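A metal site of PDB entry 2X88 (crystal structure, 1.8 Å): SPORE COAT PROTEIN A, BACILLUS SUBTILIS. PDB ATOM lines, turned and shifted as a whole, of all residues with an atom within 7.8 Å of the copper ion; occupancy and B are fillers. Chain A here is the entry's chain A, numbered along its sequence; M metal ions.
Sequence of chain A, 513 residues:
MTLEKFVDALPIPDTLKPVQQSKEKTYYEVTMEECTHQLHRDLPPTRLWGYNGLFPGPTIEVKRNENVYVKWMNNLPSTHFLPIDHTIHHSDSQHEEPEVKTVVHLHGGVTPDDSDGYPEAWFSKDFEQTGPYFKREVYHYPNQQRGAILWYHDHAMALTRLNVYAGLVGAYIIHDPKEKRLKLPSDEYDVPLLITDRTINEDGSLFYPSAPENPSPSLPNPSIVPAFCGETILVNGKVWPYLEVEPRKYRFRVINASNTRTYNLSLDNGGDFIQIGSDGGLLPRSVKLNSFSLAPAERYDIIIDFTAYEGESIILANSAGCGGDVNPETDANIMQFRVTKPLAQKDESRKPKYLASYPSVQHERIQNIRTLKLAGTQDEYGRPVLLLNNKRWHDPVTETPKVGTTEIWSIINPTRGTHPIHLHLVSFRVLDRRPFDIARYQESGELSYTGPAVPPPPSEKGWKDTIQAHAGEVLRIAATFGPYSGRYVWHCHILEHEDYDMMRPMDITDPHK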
ATOM      1  N   PRO A 226      14.751  -5.725 -16.322  1.00  0.00           N
ATOM      2  CA  PRO A 226      14.854  -6.565 -17.517  1.00  0.00           C
ATOM      3  C   PRO A 226      15.271  -8.014 -17.260  1.00  0.00           C
ATOM      4  O   PRO A 226      15.230  -8.836 -18.176  1.00  0.00           O
ATOM      5  CB  PRO A 226      15.919  -5.849 -18.357  1.00  0.00           C
ATOM      6  CG  PRO A 226      16.747  -5.123 -17.374  1.00  0.00           C
ATOM      7  CD  PRO A 226      15.829  -4.724 -16.244  1.00  0.00           C
ATOM      8  N   LEU A 374      14.333 -10.920 -33.098  1.00  0.00           N
ATOM      9  CA  LEU A 374      14.265 -10.560 -31.690  1.00  0.00           C
ATOM     10  C   LEU A 374      14.959  -9.215 -31.526  1.00  0.00           C
ATOM     11  O   LEU A 374      16.151  -9.085 -31.775  1.00  0.00           O
ATOM     12  CB  LEU A 374      14.947 -11.635 -30.827  1.00  0.00           C
ATOM     13  CG  LEU A 374      14.584 -13.105 -31.068  1.00  0.00           C
ATOM     14  CD1 LEU A 374      15.323 -14.015 -30.087  1.00  0.00           C
ATOM     15  CD2 LEU A 374      13.086 -13.356 -30.985  1.00  0.00           C
ATOM     16  N   LEU A 386      11.588  -5.125 -24.842  1.00  0.00           N
ATOM     17  CA  LEU A 386      11.927  -6.215 -25.748  1.00  0.00           C
ATOM     18  C   LEU A 386      10.732  -6.626 -26.593  1.00  0.00           C
ATOM     19  O   LEU A 386       9.621  -6.807 -26.079  1.00  0.00           O
ATOM     20  CB  LEU A 386      12.513  -7.415 -24.984  1.00  0.00           C
ATOM     21  CG  LEU A 386      13.988  -7.229 -24.620  1.00  0.00           C
ATOM     22  CD1 LEU A 386      14.409  -8.203 -23.542  1.00  0.00           C
ATOM     23  CD2 LEU A 386      14.902  -7.377 -25.836  1.00  0.00           C
ATOM     24  N   LEU A 388       9.131  -8.819 -30.235  1.00  0.00           N
ATOM     25  CA  LEU A 388       9.218  -9.807 -31.297  1.00  0.00           C
ATOM     26  C   LEU A 388       8.796  -9.125 -32.592  1.00  0.00           C
ATOM     27  O   LEU A 388       7.680  -8.618 -32.694  1.00  0.00           O
ATOM     28  CB  LEU A 388       8.308 -11.000 -31.000  1.00  0.00           C
ATOM     29  CG  LEU A 388       8.496 -11.755 -29.666  1.00  0.00           C
ATOM     30  CD1 LEU A 388       7.309 -12.667 -29.382  1.00  0.00           C
ATOM     31  CD2 LEU A 388       9.796 -12.559 -29.649  1.00  0.00           C
ATOM     32  N   ASN A 413      18.409 -13.681 -33.951  1.00  0.00           N
ATOM     33  CA  ASN A 413      18.762 -13.038 -32.684  1.00  0.00           C
ATOM     34  C   ASN A 413      20.019 -12.177 -32.777  1.00  0.00           C
ATOM     35  O   ASN A 413      21.139 -12.682 -32.616  1.00  0.00           O
ATOM     36  CB  ASN A 413      18.914 -14.094 -31.565  1.00  0.00           C
ATOM     37  CG  ASN A 413      19.192 -13.466 -30.203  1.00  0.00           C
ATOM     38  OD1 ASN A 413      19.226 -12.246 -30.053  1.00  0.00           O
ATOM     39  ND2 ASN A 413      19.384 -14.308 -29.197  1.00  0.00           N
ATOM     40  N   THR A 415      20.553  -9.726 -30.631  1.00  0.00           N
ATOM     41  CA  THR A 415      20.767  -9.174 -29.279  1.00  0.00           C
ATOM     42  C   THR A 415      22.013  -9.777 -28.628  1.00  0.00           C
ATOM     43  O   THR A 415      22.708 -10.596 -29.243  1.00  0.00           O
ATOM     44  CB  THR A 415      19.518  -9.367 -28.349  1.00  0.00           C
ATOM     45  OG1 THR A 415      19.424 -10.732 -27.922  1.00  0.00           O
ATOM     46  CG2 THR A 415      18.240  -8.946 -29.049  1.00  0.00           C
ATOM     47  N   GLY A 417      22.140 -11.562 -25.706  1.00  0.00           N
ATOM     48  CA  GLY A 417      21.904 -12.756 -24.890  1.00  0.00           C
ATOM     49  C   GLY A 417      20.999 -13.793 -25.541  1.00  0.00           C
ATOM     50  O   GLY A 417      20.415 -13.550 -26.598  1.00  0.00           O
ATOM     51  N   THR A 418      20.907 -14.948 -24.894  1.00  0.00           N
ATOM     52  CA  THR A 418      20.024 -16.033 -25.322  1.00  0.00           C
ATOM     53  C   THR A 418      18.589 -15.735 -24.867  1.00  0.00           C
ATOM     54  O   THR A 418      18.377 -15.216 -23.768  1.00  0.00           O
ATOM     55  CB  THR A 418      20.481 -17.390 -24.726  1.00  0.00           C
ATOM     56  OG1 THR A 418      21.806 -17.680 -25.170  1.00  0.00           O
ATOM     57  CG2 THR A 418      19.559 -18.525 -25.169  1.00  0.00           C
ATOM     58  N   HIS A 419      17.627 -16.056 -25.725  1.00  0.00           N
ATOM     59  CA  HIS A 419      16.212 -15.979 -25.377  1.00  0.00           C
ATOM     60  C   HIS A 419      15.587 -17.360 -25.566  1.00  0.00           C
ATOM     61  O   HIS A 419      15.672 -17.928 -26.647  1.00  0.00           O
ATOM     62  CB  HIS A 419      15.480 -14.934 -26.237  1.00  0.00           C
ATOM     63  CG  HIS A 419      16.042 -13.549 -26.127  1.00  0.00           C
ATOM     64  ND1 HIS A 419      15.603 -12.651 -25.173  1.00  0.00           N
ATOM     65  CD2 HIS A 419      16.987 -12.905 -26.846  1.00  0.00           C
ATOM     66  CE1 HIS A 419      16.265 -11.516 -25.313  1.00  0.00           C
ATOM     67  NE2 HIS A 419      17.106 -11.642 -26.326  1.00  0.00           N
ATOM     68  N   PRO A 420      14.966 -17.908 -24.503  1.00  0.00           N
ATOM     69  CA  PRO A 420      14.261 -19.183 -24.642  1.00  0.00           C
ATOM     70  C   PRO A 420      12.866 -18.950 -25.222  1.00  0.00           C
ATOM     71  O   PRO A 420      11.952 -18.516 -24.519  1.00  0.00           O
ATOM     72  CB  PRO A 420      14.202 -19.709 -23.198  1.00  0.00           C
ATOM     73  CG  PRO A 420      14.184 -18.475 -22.355  1.00  0.00           C
ATOM     74  CD  PRO A 420      14.948 -17.414 -23.110  1.00  0.00           C
ATOM     75  N   ILE A 421      12.723 -19.212 -26.514  1.00  0.00           N
ATOM     76  CA  ILE A 421      11.482 -18.939 -27.235  1.00  0.00           C
ATOM     77  C   ILE A 421      10.515 -20.104 -27.102  1.00  0.00           C
ATOM     78  O   ILE A 421      10.872 -21.261 -27.333  1.00  0.00           O
ATOM     79  CB  ILE A 421      11.746 -18.623 -28.744  1.00  0.00           C
ATOM     80  CG1 ILE A 421      12.724 -17.443 -28.892  1.00  0.00           C
ATOM     81  CG2 ILE A 421      10.430 -18.380 -29.508  1.00  0.00           C
ATOM     82  CD1 ILE A 421      12.247 -16.116 -28.283  1.00  0.00           C
ATOM     83  N   HIS A 491       6.240 -16.488 -27.280  1.00  0.00           N
ATOM     84  CA  HIS A 491       6.984 -15.506 -26.483  1.00  0.00           C
ATOM     85  C   HIS A 491       8.325 -16.012 -25.987  1.00  0.00           C
ATOM     86  O   HIS A 491       8.601 -17.222 -26.005  1.00  0.00           O
ATOM     87  CB  HIS A 491       6.144 -15.046 -25.282  1.00  0.00           C
ATOM     88  CG  HIS A 491       5.750 -16.145 -24.345  1.00  0.00           C
ATOM     89  ND1 HIS A 491       6.482 -16.463 -23.217  1.00  0.00           N
ATOM     90  CD2 HIS A 491       4.694 -16.993 -24.370  1.00  0.00           C
ATOM     91  CE1 HIS A 491       5.894 -17.468 -22.590  1.00  0.00           C
ATOM     92  NE2 HIS A 491       4.812 -17.800 -23.263  1.00  0.00           N
ATOM     93  N   CYS A 492       9.168 -15.086 -25.531  1.00  0.00           N
ATOM     94  CA  CYS A 492      10.327 -15.441 -24.738  1.00  0.00           C
ATOM     95  C   CYS A 492       9.849 -15.825 -23.340  1.00  0.00           C
ATOM     96  O   CYS A 492       8.945 -15.178 -22.789  1.00  0.00           O
ATOM     97  CB  CYS A 492      11.295 -14.265 -24.641  1.00  0.00           C
ATOM     98  SG  CYS A 492      12.700 -14.557 -23.562  1.00  0.00           S
ATOM     99  N   HIS A 493      10.431 -16.875 -22.767  1.00  0.00           N
ATOM    100  CA  HIS A 493      10.002 -17.365 -21.458  1.00  0.00           C
ATOM    101  C   HIS A 493      10.888 -16.852 -20.298  1.00  0.00           C
ATOM    102  O   HIS A 493      10.806 -17.361 -19.171  1.00  0.00           O
ATOM    103  CB  HIS A 493       9.890 -18.893 -21.436  1.00  0.00           C
ATOM    104  CG  HIS A 493       8.790 -19.421 -20.558  1.00  0.00           C
ATOM    105  ND1 HIS A 493       8.816 -19.295 -19.185  1.00  0.00           N
ATOM    106  CD2 HIS A 493       7.648 -20.068 -20.856  1.00  0.00           C
ATOM    107  CE1 HIS A 493       7.727 -19.844 -18.679  1.00  0.00           C
ATOM    108  NE2 HIS A 493       7.001 -20.322 -19.670  1.00  0.00           N
ATOM    109  N   ILE A 494      11.717 -15.856 -20.570  1.00  0.00           N
ATOM    110  CA  ILE A 494      12.282 -15.033 -19.500  1.00  0.00           C
ATOM    111  C   ILE A 494      11.129 -14.098 -19.127  1.00  0.00           C
ATOM    112  O   ILE A 494      10.706 -13.273 -19.939  1.00  0.00           O
ATOM    113  CB  ILE A 494      13.549 -14.243 -19.927  1.00  0.00           C
ATOM    114  CG1 ILE A 494      14.725 -15.202 -20.131  1.00  0.00           C
ATOM    115  CG2 ILE A 494      13.903 -13.171 -18.871  1.00  0.00           C
ATOM    116  CD1 ILE A 494      15.896 -14.611 -20.907  1.00  0.00           C
ATOM    117  N   LEU A 495      10.610 -14.260 -17.919  1.00  0.00           N
ATOM    118  CA  LEU A 495       9.339 -13.634 -17.554  1.00  0.00           C
ATOM    119  C   LEU A 495       9.416 -12.117 -17.528  1.00  0.00           C
ATOM    120  O   LEU A 495       8.436 -11.442 -17.845  1.00  0.00           O
ATOM    121  CB  LEU A 495       8.816 -14.200 -16.225  1.00  0.00           C
ATOM    122  CG  LEU A 495       8.622 -15.722 -16.166  1.00  0.00           C
ATOM    123  CD1 LEU A 495       7.953 -16.108 -14.859  1.00  0.00           C
ATOM    124  CD2 LEU A 495       7.806 -16.257 -17.348  1.00  0.00           C
ATOM    125  N   GLU A 496      10.586 -11.596 -17.173  1.00  0.00           N
ATOM    126  CA  GLU A 496      10.855 -10.165 -17.202  1.00  0.00           C
ATOM    127  C   GLU A 496      10.827  -9.606 -18.633  1.00  0.00           C
ATOM    128  O   GLU A 496      10.518  -8.426 -18.841  1.00  0.00           O
ATOM    129  CB  GLU A 496      12.188  -9.860 -16.524  1.00  0.00           C
ATOM    130  CG  GLU A 496      12.143  -9.897 -14.980  1.00  0.00           C
ATOM    131  CD  GLU A 496      12.006 -11.289 -14.385  1.00  0.00           C
ATOM    132  OE1 GLU A 496      12.396 -12.286 -15.036  1.00  0.00           O
ATOM    133  OE2 GLU A 496      11.501 -11.397 -13.243  1.00  0.00           O
ATOM    134  N   HIS A 497      11.145 -10.451 -19.611  1.00  0.00           N
ATOM    135  CA  HIS A 497      11.062 -10.063 -21.023  1.00  0.00           C
ATOM    136  C   HIS A 497       9.636 -10.190 -21.536  1.00  0.00           C
ATOM    137  O   HIS A 497       9.126  -9.292 -22.203  1.00  0.00           O
ATOM    138  CB  HIS A 497      11.988 -10.916 -21.905  1.00  0.00           C
ATOM    139  CG  HIS A 497      13.441 -10.753 -21.590  1.00  0.00           C
ATOM    140  ND1 HIS A 497      14.419 -11.471 -22.247  1.00  0.00           N
ATOM    141  CD2 HIS A 497      14.079  -9.989 -20.681  1.00  0.00           C
ATOM    142  CE1 HIS A 497      15.603 -11.140 -21.759  1.00  0.00           C
ATOM    143  NE2 HIS A 497      15.429 -10.238 -20.811  1.00  0.00           N
ATOM    144  N   GLU A 498       8.997 -11.322 -21.212  1.00  0.00           N
ATOM    145  CA  GLU A 498       7.616 -11.620 -21.597  1.00  0.00           C
ATOM    146  C   GLU A 498       6.654 -10.490 -21.225  1.00  0.00           C
ATOM    147  O   GLU A 498       5.809 -10.103 -22.028  1.00  0.00           O
ATOM    148  CB  GLU A 498       7.173 -12.937 -20.952  1.00  0.00           C
ATOM    149  CG  GLU A 498       5.719 -13.334 -21.193  1.00  0.00           C
ATOM    150  CD  GLU A 498       5.369 -14.649 -20.521  1.00  0.00           C
ATOM    151  OE1 GLU A 498       6.292 -15.447 -20.236  1.00  0.00           O
ATOM    152  OE2 GLU A 498       4.172 -14.891 -20.287  1.00  0.00           O
ATOM    153  N   MET A 502       7.809  -8.938 -24.767  1.00  0.00           N
ATOM    154  CA  MET A 502       8.304  -9.924 -25.736  1.00  0.00           C
ATOM    155  C   MET A 502       7.345 -11.105 -25.885  1.00  0.00           C
ATOM    156  O   MET A 502       7.719 -12.272 -25.687  1.00  0.00           O
ATOM    157  CB  MET A 502       9.708 -10.386 -25.326  1.00  0.00           C
ATOM    158  CG  MET A 502      10.586 -10.849 -26.474  1.00  0.00           C
ATOM    159  SD  MET A 502      12.284 -11.108 -25.929  1.00  0.00           S
ATOM    160  CE  MET A 502      13.038 -11.760 -27.416  1.00  0.00           C
HETATM  161 CU    CU M   1      14.081 -12.839 -23.762  1.00  0.00          CU
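Merely in contact with the copper ion: Ile 494 (3.8 Å) and Met 502 (3.3 Å).
Within 4 Å of the copper ion: His 419, Cys 492, Ile 494, His 497 and Met 502.
The nearest printed residue that does not touch the copper ion is Leu 386 (4.7 Å).
O of His 497 sits at hydrogen-bond distance from N of Met 502 (2.9 Å).
The backbone carbonyl oxygen (O) of Pro 226 lies close to a ring nitrogen (NE2) of His 497 (3.0 Å).
ND1 of His 419 lies close to SD of Met 502, 3.7 Å away.
The side-chain hydroxyl (OG1) of Thr 415 sits at hydrogen-bond distance from a ring nitrogen (NE2) of His 419, 3.0 Å away.
The backbone NH (N) of Cys 492 lies within hydrogen-bond range of the backbone carbonyl oxygen (O) of Met 502 (3.2 Å).
The side-chain sulfur (SG) of Cys 492 lies close to the backbone NH (N) of Ile 494, at 3.4 Å.
O of Leu 386 lies within hydrogen-bond range of N of Met 502, at 3.1 Å.
The copper ion is bound by ND1 of His 497 (2.1 Å).
ND1 of His 419 binds the copper ion (2.1 Å).
SG of Cys 492 binds the copper ion, 2.2 Å away.
The copper ion has three donor atoms within binding distance.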
